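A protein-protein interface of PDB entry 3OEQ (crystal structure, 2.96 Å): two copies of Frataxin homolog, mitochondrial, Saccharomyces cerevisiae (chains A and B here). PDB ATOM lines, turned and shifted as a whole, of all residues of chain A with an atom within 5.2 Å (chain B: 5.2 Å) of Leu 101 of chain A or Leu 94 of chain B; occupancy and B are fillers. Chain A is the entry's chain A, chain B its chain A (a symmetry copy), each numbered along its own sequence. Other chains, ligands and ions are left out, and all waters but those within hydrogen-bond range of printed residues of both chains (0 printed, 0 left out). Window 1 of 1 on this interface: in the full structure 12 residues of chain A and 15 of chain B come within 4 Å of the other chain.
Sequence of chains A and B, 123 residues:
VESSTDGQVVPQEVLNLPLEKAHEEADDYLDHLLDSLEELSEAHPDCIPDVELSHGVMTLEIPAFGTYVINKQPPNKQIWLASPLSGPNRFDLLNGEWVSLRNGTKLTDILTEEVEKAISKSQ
NH1 of Arg 90 of chain A is in salt-bridge range of OE2 of Glu 25 of chain B (3.7 Å). The backbone NH (N) of Gly 96 of chain B is in hydrogen-bond range of the backbone carbonyl oxygen (O) of Leu 101 of chain A (3.0 Å). O of Arg 102 of chain A is in hydrogen-bond range of N of Gly 96 of chain B, 2.9 Å away. The backbone carbonyl oxygen of Leu 101 of chain A sits close to the backbone carbonyl oxygen of Leu 94 of chain B (2.9 Å). O of Arg 102 of chain A lies close to O of Asn 95 of chain B (3.3 Å).
The guanidinium group (NE) of Arg 90 of chain A sits at hydrogen-bond distance from the backbone carbonyl oxygen (O) of Lys 77 of chain A (2.9 Å). NH2 of Arg 102 of chain A sits close to ND2 of Asn 89 of chain A (3.2 Å). The backbone NH of Leu 101 of chain A sits at hydrogen-bond distance from the backbone carbonyl oxygen of Arg 90 of chain A (3.0 Å). The side-chain hydroxyl of Ser 100 of chain A is in hydrogen-bond range of the backbone NH of Arg 102 of chain A (3.1 Å). The backbone NH (N) of Asn 103 of chain A sits at hydrogen-bond distance from the side-chain hydroxyl (OG) of Ser 100 of chain A. O of Val 99 of chain B sits at hydrogen-bond distance from N of Asp 92 of chain B, 2.9 Å away.
Leu 101 of chain A touches just these residues of chain B: Leu 94, Asn 95 and Gly 96. Of the printed residues of chain B, Asn 103 of chain A touches Asn 95 (3.9 Å). Of the printed residues of chain A, Asn 95 of chain B touches Leu 101, Arg 102 and Asn 103. Printed residues of chain B within 4 Å of Asn 76 of chain A: Asp 92 (3.8 Å). Asn 89 of chain A touches none of the printed residues of chain B. The nearest residue of chain B that does not touch Leu 101 of chain A is Leu 93 of chain B (4.2 Å).
Among the printed residues, pairs that only touch across the chains: Leu 101 of chain A with Asn 95 of chain B (3.4 Å), Asn 76 of chain A with Asp 92 of chain B (3.8 Å) and Asn 103 of chain A with Asn 95 of chain B (3.9 Å).
Of the 8 printed residues of chain B, 5 touch a printed residue of chain A. Printed residues of chain B that touch a printed residue of chain A: Glu 25, Asp 92, Leu 94, Asn 95 and Gly 96.
2 positions are printed for both chains. Of the 8 pairs that touch across the chains among the printed residues, none has its exchanged pair printed and touching as well.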
ATOM      1  N   ASN A  76     -17.178 -32.456  20.082  1.00  0.00           N
ATOM      2  CA  ASN A  76     -17.284 -31.084  20.637  1.00  0.00           C
ATOM      3  C   ASN A  76     -16.398 -30.167  19.886  1.00  0.00           C
ATOM      4  O   ASN A  76     -16.539 -28.958  20.004  1.00  0.00           O
ATOM      5  CB  ASN A  76     -17.040 -31.040  22.089  1.00  0.00           C
ATOM      6  CG  ASN A  76     -18.214 -31.593  22.785  1.00  0.00           C
ATOM      7  OD1 ASN A  76     -19.117 -32.028  22.112  1.00  0.00           O
ATOM      8  ND2 ASN A  76     -18.256 -31.549  24.116  1.00  0.00           N
ATOM      9  N   LYS A  77     -15.589 -30.867  19.050  1.00  0.00           N
ATOM     10  CA  LYS A  77     -14.616 -30.496  17.989  1.00  0.00           C
ATOM     11  C   LYS A  77     -13.372 -31.398  18.202  1.00  0.00           C
ATOM     12  O   LYS A  77     -12.972 -31.594  19.347  1.00  0.00           O
ATOM     13  N   ASN A  89      -5.276 -25.354  21.480  1.00  0.00           N
ATOM     14  CA  ASN A  89      -6.350 -25.137  20.494  1.00  0.00           C
ATOM     15  C   ASN A  89      -7.046 -26.414  20.018  1.00  0.00           C
ATOM     16  O   ASN A  89      -6.478 -27.469  20.148  1.00  0.00           O
ATOM     17  CB  ASN A  89      -5.862 -24.252  19.321  1.00  0.00           C
ATOM     18  CG  ASN A  89      -6.773 -23.047  19.101  1.00  0.00           C
ATOM     19  OD1 ASN A  89      -7.946 -23.181  18.694  1.00  0.00           O
ATOM     20  ND2 ASN A  89      -6.277 -21.882  19.446  1.00  0.00           N
ATOM     21  N   ARG A  90      -8.276 -26.331  19.511  1.00  0.00           N
ATOM     22  CA  ARG A  90      -8.869 -27.502  18.837  1.00  0.00           C
ATOM     23  C   ARG A  90      -9.503 -27.251  17.478  1.00  0.00           C
ATOM     24  O   ARG A  90      -9.956 -26.173  17.210  1.00  0.00           O
ATOM     25  CB  ARG A  90      -9.762 -28.361  19.756  1.00  0.00           C
ATOM     26  CG  ARG A  90     -11.147 -27.860  19.970  1.00  0.00           C
ATOM     27  CD  ARG A  90     -11.645 -28.279  21.329  1.00  0.00           C
ATOM     28  NE  ARG A  90     -12.067 -29.658  21.344  1.00  0.00           N
ATOM     29  CZ  ARG A  90     -11.825 -30.501  22.328  1.00  0.00           C
ATOM     30  NH1 ARG A  90     -11.131 -30.111  23.358  1.00  0.00           N
ATOM     31  NH2 ARG A  90     -12.223 -31.754  22.247  1.00  0.00           N
ATOM     32  N   PHE A  91      -9.519 -28.290  16.646  1.00  0.00           N
ATOM     33  CA  PHE A  91      -9.692 -28.148  15.226  1.00  0.00           C
ATOM     34  C   PHE A  91     -10.687 -29.136  14.585  1.00  0.00           C
ATOM     35  O   PHE A  91     -10.598 -30.335  14.793  1.00  0.00           O
ATOM     36  CB  PHE A  91      -8.319 -28.317  14.550  1.00  0.00           C
ATOM     37  CG  PHE A  91      -7.292 -27.328  15.012  1.00  0.00           C
ATOM     38  CD1 PHE A  91      -7.217 -26.080  14.437  1.00  0.00           C
ATOM     39  CD2 PHE A  91      -6.428 -27.635  16.048  1.00  0.00           C
ATOM     40  CE1 PHE A  91      -6.309 -25.161  14.879  1.00  0.00           C
ATOM     41  CE2 PHE A  91      -5.511 -26.718  16.498  1.00  0.00           C
ATOM     42  CZ  PHE A  91      -5.436 -25.487  15.908  1.00  0.00           C
ATOM     43  N   ASP A  92     -11.575 -28.643  13.718  1.00  0.00           N
ATOM     44  CA  ASP A  92     -12.398 -29.556  12.924  1.00  0.00           C
ATOM     45  C   ASP A  92     -12.265 -29.274  11.439  1.00  0.00           C
ATOM     46  O   ASP A  92     -11.918 -28.163  11.045  1.00  0.00           O
ATOM     47  CB  ASP A  92     -13.860 -29.457  13.348  1.00  0.00           C
ATOM     48  CG  ASP A  92     -14.454 -30.804  13.720  1.00  0.00           C
ATOM     49  OD1 ASP A  92     -15.043 -30.893  14.817  1.00  0.00           O
ATOM     50  OD2 ASP A  92     -14.326 -31.774  12.942  1.00  0.00           O
ATOM     51  N   VAL A  99      -9.195 -26.651  11.034  1.00  0.00           N
ATOM     52  CA  VAL A  99      -9.487 -25.269  11.332  1.00  0.00           C
ATOM     53  C   VAL A  99      -9.882 -25.126  12.780  1.00  0.00           C
ATOM     54  O   VAL A  99     -10.604 -25.933  13.326  1.00  0.00           O
ATOM     55  CB  VAL A  99     -10.606 -24.774  10.374  1.00  0.00           C
ATOM     56  CG1 VAL A  99     -11.719 -24.011  11.086  1.00  0.00           C
ATOM     57  CG2 VAL A  99      -9.996 -24.007   9.205  1.00  0.00           C
ATOM     58  N   SER A 100      -9.360 -24.087  13.397  1.00  0.00           N
ATOM     59  CA  SER A 100      -9.640 -23.734  14.780  1.00  0.00           C
ATOM     60  C   SER A 100     -11.101 -23.359  15.075  1.00  0.00           C
ATOM     61  O   SER A 100     -11.685 -22.512  14.420  1.00  0.00           O
ATOM     62  CB  SER A 100      -8.697 -22.603  15.173  1.00  0.00           C
ATOM     63  OG  SER A 100      -9.252 -21.785  16.164  1.00  0.00           O
ATOM     64  N   LEU A 101     -11.673 -24.004  16.082  1.00  0.00           N
ATOM     65  CA  LEU A 101     -12.984 -23.616  16.613  1.00  0.00           C
ATOM     66  C   LEU A 101     -12.960 -22.194  17.153  1.00  0.00           C
ATOM     67  O   LEU A 101     -13.883 -21.442  16.908  1.00  0.00           O
ATOM     68  CB  LEU A 101     -13.494 -24.611  17.660  1.00  0.00           C
ATOM     69  CG  LEU A 101     -13.683 -26.066  17.187  1.00  0.00           C
ATOM     70  CD1 LEU A 101     -14.114 -26.962  18.323  1.00  0.00           C
ATOM     71  CD2 LEU A 101     -14.651 -26.222  16.043  1.00  0.00           C
ATOM     72  N   ARG A 102     -11.877 -21.822  17.829  1.00  0.00           N
ATOM     73  CA  ARG A 102     -11.704 -20.460  18.335  1.00  0.00           C
ATOM     74  C   ARG A 102     -11.899 -19.328  17.300  1.00  0.00           C
ATOM     75  O   ARG A 102     -12.754 -18.481  17.503  1.00  0.00           O
ATOM     76  CB  ARG A 102     -10.383 -20.329  19.093  1.00  0.00           C
ATOM     77  CG  ARG A 102      -9.980 -18.906  19.465  1.00  0.00           C
ATOM     78  CD  ARG A 102      -9.351 -18.799  20.854  1.00  0.00           C
ATOM     79  NE  ARG A 102      -8.324 -19.810  21.103  1.00  0.00           N
ATOM     80  CZ  ARG A 102      -8.082 -20.340  22.303  1.00  0.00           C
ATOM     81  NH1 ARG A 102      -8.781 -19.992  23.382  1.00  0.00           N
ATOM     82  NH2 ARG A 102      -7.134 -21.245  22.426  1.00  0.00           N
ATOM     83  N   ASN A 103     -11.133 -19.319  16.203  1.00  0.00           N
ATOM     84  CA  ASN A 103     -11.141 -18.237  15.198  1.00  0.00           C
ATOM     85  C   ASN A 103     -11.066 -18.756  13.767  1.00  0.00           C
ATOM     86  O   ASN A 103     -11.132 -17.987  12.813  1.00  0.00           O
ATOM     87  CB  ASN A 103      -9.985 -17.258  15.424  1.00  0.00           C
ATOM     88  CG  ASN A 103      -8.635 -17.966  15.648  1.00  0.00           C
ATOM     89  OD1 ASN A 103      -8.175 -18.767  14.833  1.00  0.00           O
ATOM     90  ND2 ASN A 103      -8.007 -17.663  16.762  1.00  0.00           N
ATOM     91  N   GLY A 104     -10.897 -20.056  13.601  1.00  0.00           N
ATOM     92  CA  GLY A 104     -10.962 -20.610  12.260  1.00  0.00           C
ATOM     93  C   GLY A 104      -9.688 -20.570  11.466  1.00  0.00           C
ATOM     94  O   GLY A 104      -9.717 -20.745  10.264  1.00  0.00           O
ATOM     95  N   GLU B  25     -15.755 -26.671  26.372  1.00  0.00           N
ATOM     96  CA  GLU B  25     -16.108 -25.335  26.001  1.00  0.00           C
ATOM     97  C   GLU B  25     -17.590 -25.052  26.270  1.00  0.00           C
ATOM     98  O   GLU B  25     -17.995 -23.926  26.578  1.00  0.00           O
ATOM     99  CB  GLU B  25     -15.712 -25.109  24.561  1.00  0.00           C
ATOM    100  CG  GLU B  25     -15.462 -26.406  23.827  1.00  0.00           C
ATOM    101  CD  GLU B  25     -14.047 -26.870  23.919  1.00  0.00           C
ATOM    102  OE1 GLU B  25     -13.172 -26.231  23.294  1.00  0.00           O
ATOM    103  OE2 GLU B  25     -13.821 -27.883  24.596  1.00  0.00           O
ATOM    104  N   ASP B  92     -23.177 -25.413  17.882  1.00  0.00           N
ATOM    105  CA  ASP B  92     -21.745 -25.709  17.952  1.00  0.00           C
ATOM    106  C   ASP B  92     -20.911 -24.451  17.788  1.00  0.00           C
ATOM    107  O   ASP B  92     -21.371 -23.472  17.205  1.00  0.00           O
ATOM    108  CB  ASP B  92     -21.363 -26.736  16.891  1.00  0.00           C
ATOM    109  CG  ASP B  92     -20.645 -27.940  17.475  1.00  0.00           C
ATOM    110  OD1 ASP B  92     -21.076 -29.072  17.173  1.00  0.00           O
ATOM    111  OD2 ASP B  92     -19.671 -27.770  18.240  1.00  0.00           O
ATOM    112  N   LEU B  93     -19.679 -24.473  18.293  1.00  0.00           N
ATOM    113  CA  LEU B  93     -18.736 -23.373  18.025  1.00  0.00           C
ATOM    114  C   LEU B  93     -18.522 -23.122  16.519  1.00  0.00           C
ATOM    115  O   LEU B  93     -18.432 -24.065  15.752  1.00  0.00           O
ATOM    116  CB  LEU B  93     -17.412 -23.610  18.740  1.00  0.00           C
ATOM    117  CG  LEU B  93     -17.545 -23.606  20.243  1.00  0.00           C
ATOM    118  CD1 LEU B  93     -16.396 -24.375  20.895  1.00  0.00           C
ATOM    119  CD2 LEU B  93     -17.676 -22.174  20.769  1.00  0.00           C
ATOM    120  N   LEU B  94     -18.495 -21.854  16.096  1.00  0.00           N
ATOM    121  CA  LEU B  94     -18.014 -21.544  14.745  1.00  0.00           C
ATOM    122  C   LEU B  94     -16.739 -20.805  14.889  1.00  0.00           C
ATOM    123  O   LEU B  94     -15.663 -21.343  14.619  1.00  0.00           O
ATOM    124  CB  LEU B  94     -18.989 -20.751  13.877  1.00  0.00           C
ATOM    125  CG  LEU B  94     -18.655 -20.633  12.382  1.00  0.00           C
ATOM    126  CD1 LEU B  94     -17.990 -21.866  11.775  1.00  0.00           C
ATOM    127  CD2 LEU B  94     -19.926 -20.323  11.639  1.00  0.00           C
ATOM    128  N   ASN B  95     -16.836 -19.570  15.332  1.00  0.00           N
ATOM    129  CA  ASN B  95     -15.622 -18.818  15.560  1.00  0.00           C
ATOM    130  C   ASN B  95     -15.655 -18.291  16.944  1.00  0.00           C
ATOM    131  O   ASN B  95     -15.775 -17.109  17.128  1.00  0.00           O
ATOM    132  CB  ASN B  95     -15.458 -17.674  14.556  1.00  0.00           C
ATOM    133  CG  ASN B  95     -15.040 -18.146  13.168  1.00  0.00           C
ATOM    134  OD1 ASN B  95     -14.801 -19.323  12.914  1.00  0.00           O
ATOM    135  ND2 ASN B  95     -14.957 -17.210  12.260  1.00  0.00           N
ATOM    136  N   GLY B  96     -15.567 -19.183  17.918  1.00  0.00           N
ATOM    137  CA  GLY B  96     -15.545 -18.791  19.302  1.00  0.00           C
ATOM    138  C   GLY B  96     -16.914 -18.516  19.865  1.00  0.00           C
ATOM    139  O   GLY B  96     -17.051 -18.407  21.065  1.00  0.00           O
ATOM    140  N   GLU B  97     -17.938 -18.390  19.028  1.00  0.00           N
ATOM    141  CA  GLU B  97     -19.297 -18.294  19.583  1.00  0.00           C
ATOM    142  C   GLU B  97     -20.250 -19.424  19.147  1.00  0.00           C
ATOM    143  O   GLU B  97     -20.038 -20.068  18.133  1.00  0.00           O
ATOM    144  CB  GLU B  97     -19.897 -16.863  19.476  1.00  0.00           C
ATOM    145  CG  GLU B  97     -21.115 -16.532  20.449  1.00  0.00           C
ATOM    146  CD  GLU B  97     -20.796 -16.416  21.940  1.00  0.00           C
ATOM    147  OE1 GLU B  97     -20.756 -15.277  22.444  1.00  0.00           O
ATOM    148  OE2 GLU B  97     -20.637 -17.449  22.604  1.00  0.00           O
ATOM    149  N   VAL B  99     -23.489 -21.323  17.977  1.00  0.00           N
ATOM    150  CA  VAL B  99     -24.252 -21.047  16.783  1.00  0.00           C
ATOM    151  C   VAL B  99     -25.145 -22.217  16.458  1.00  0.00           C
ATOM    152  O   VAL B  99     -24.758 -23.362  16.567  1.00  0.00           O
ATOM    153  CB  VAL B  99     -23.270 -20.727  15.622  1.00  0.00           C
ATOM    154  CG1 VAL B  99     -23.600 -21.465  14.329  1.00  0.00           C
ATOM    155  CG2 VAL B  99     -23.142 -19.217  15.443  1.00  0.00           C
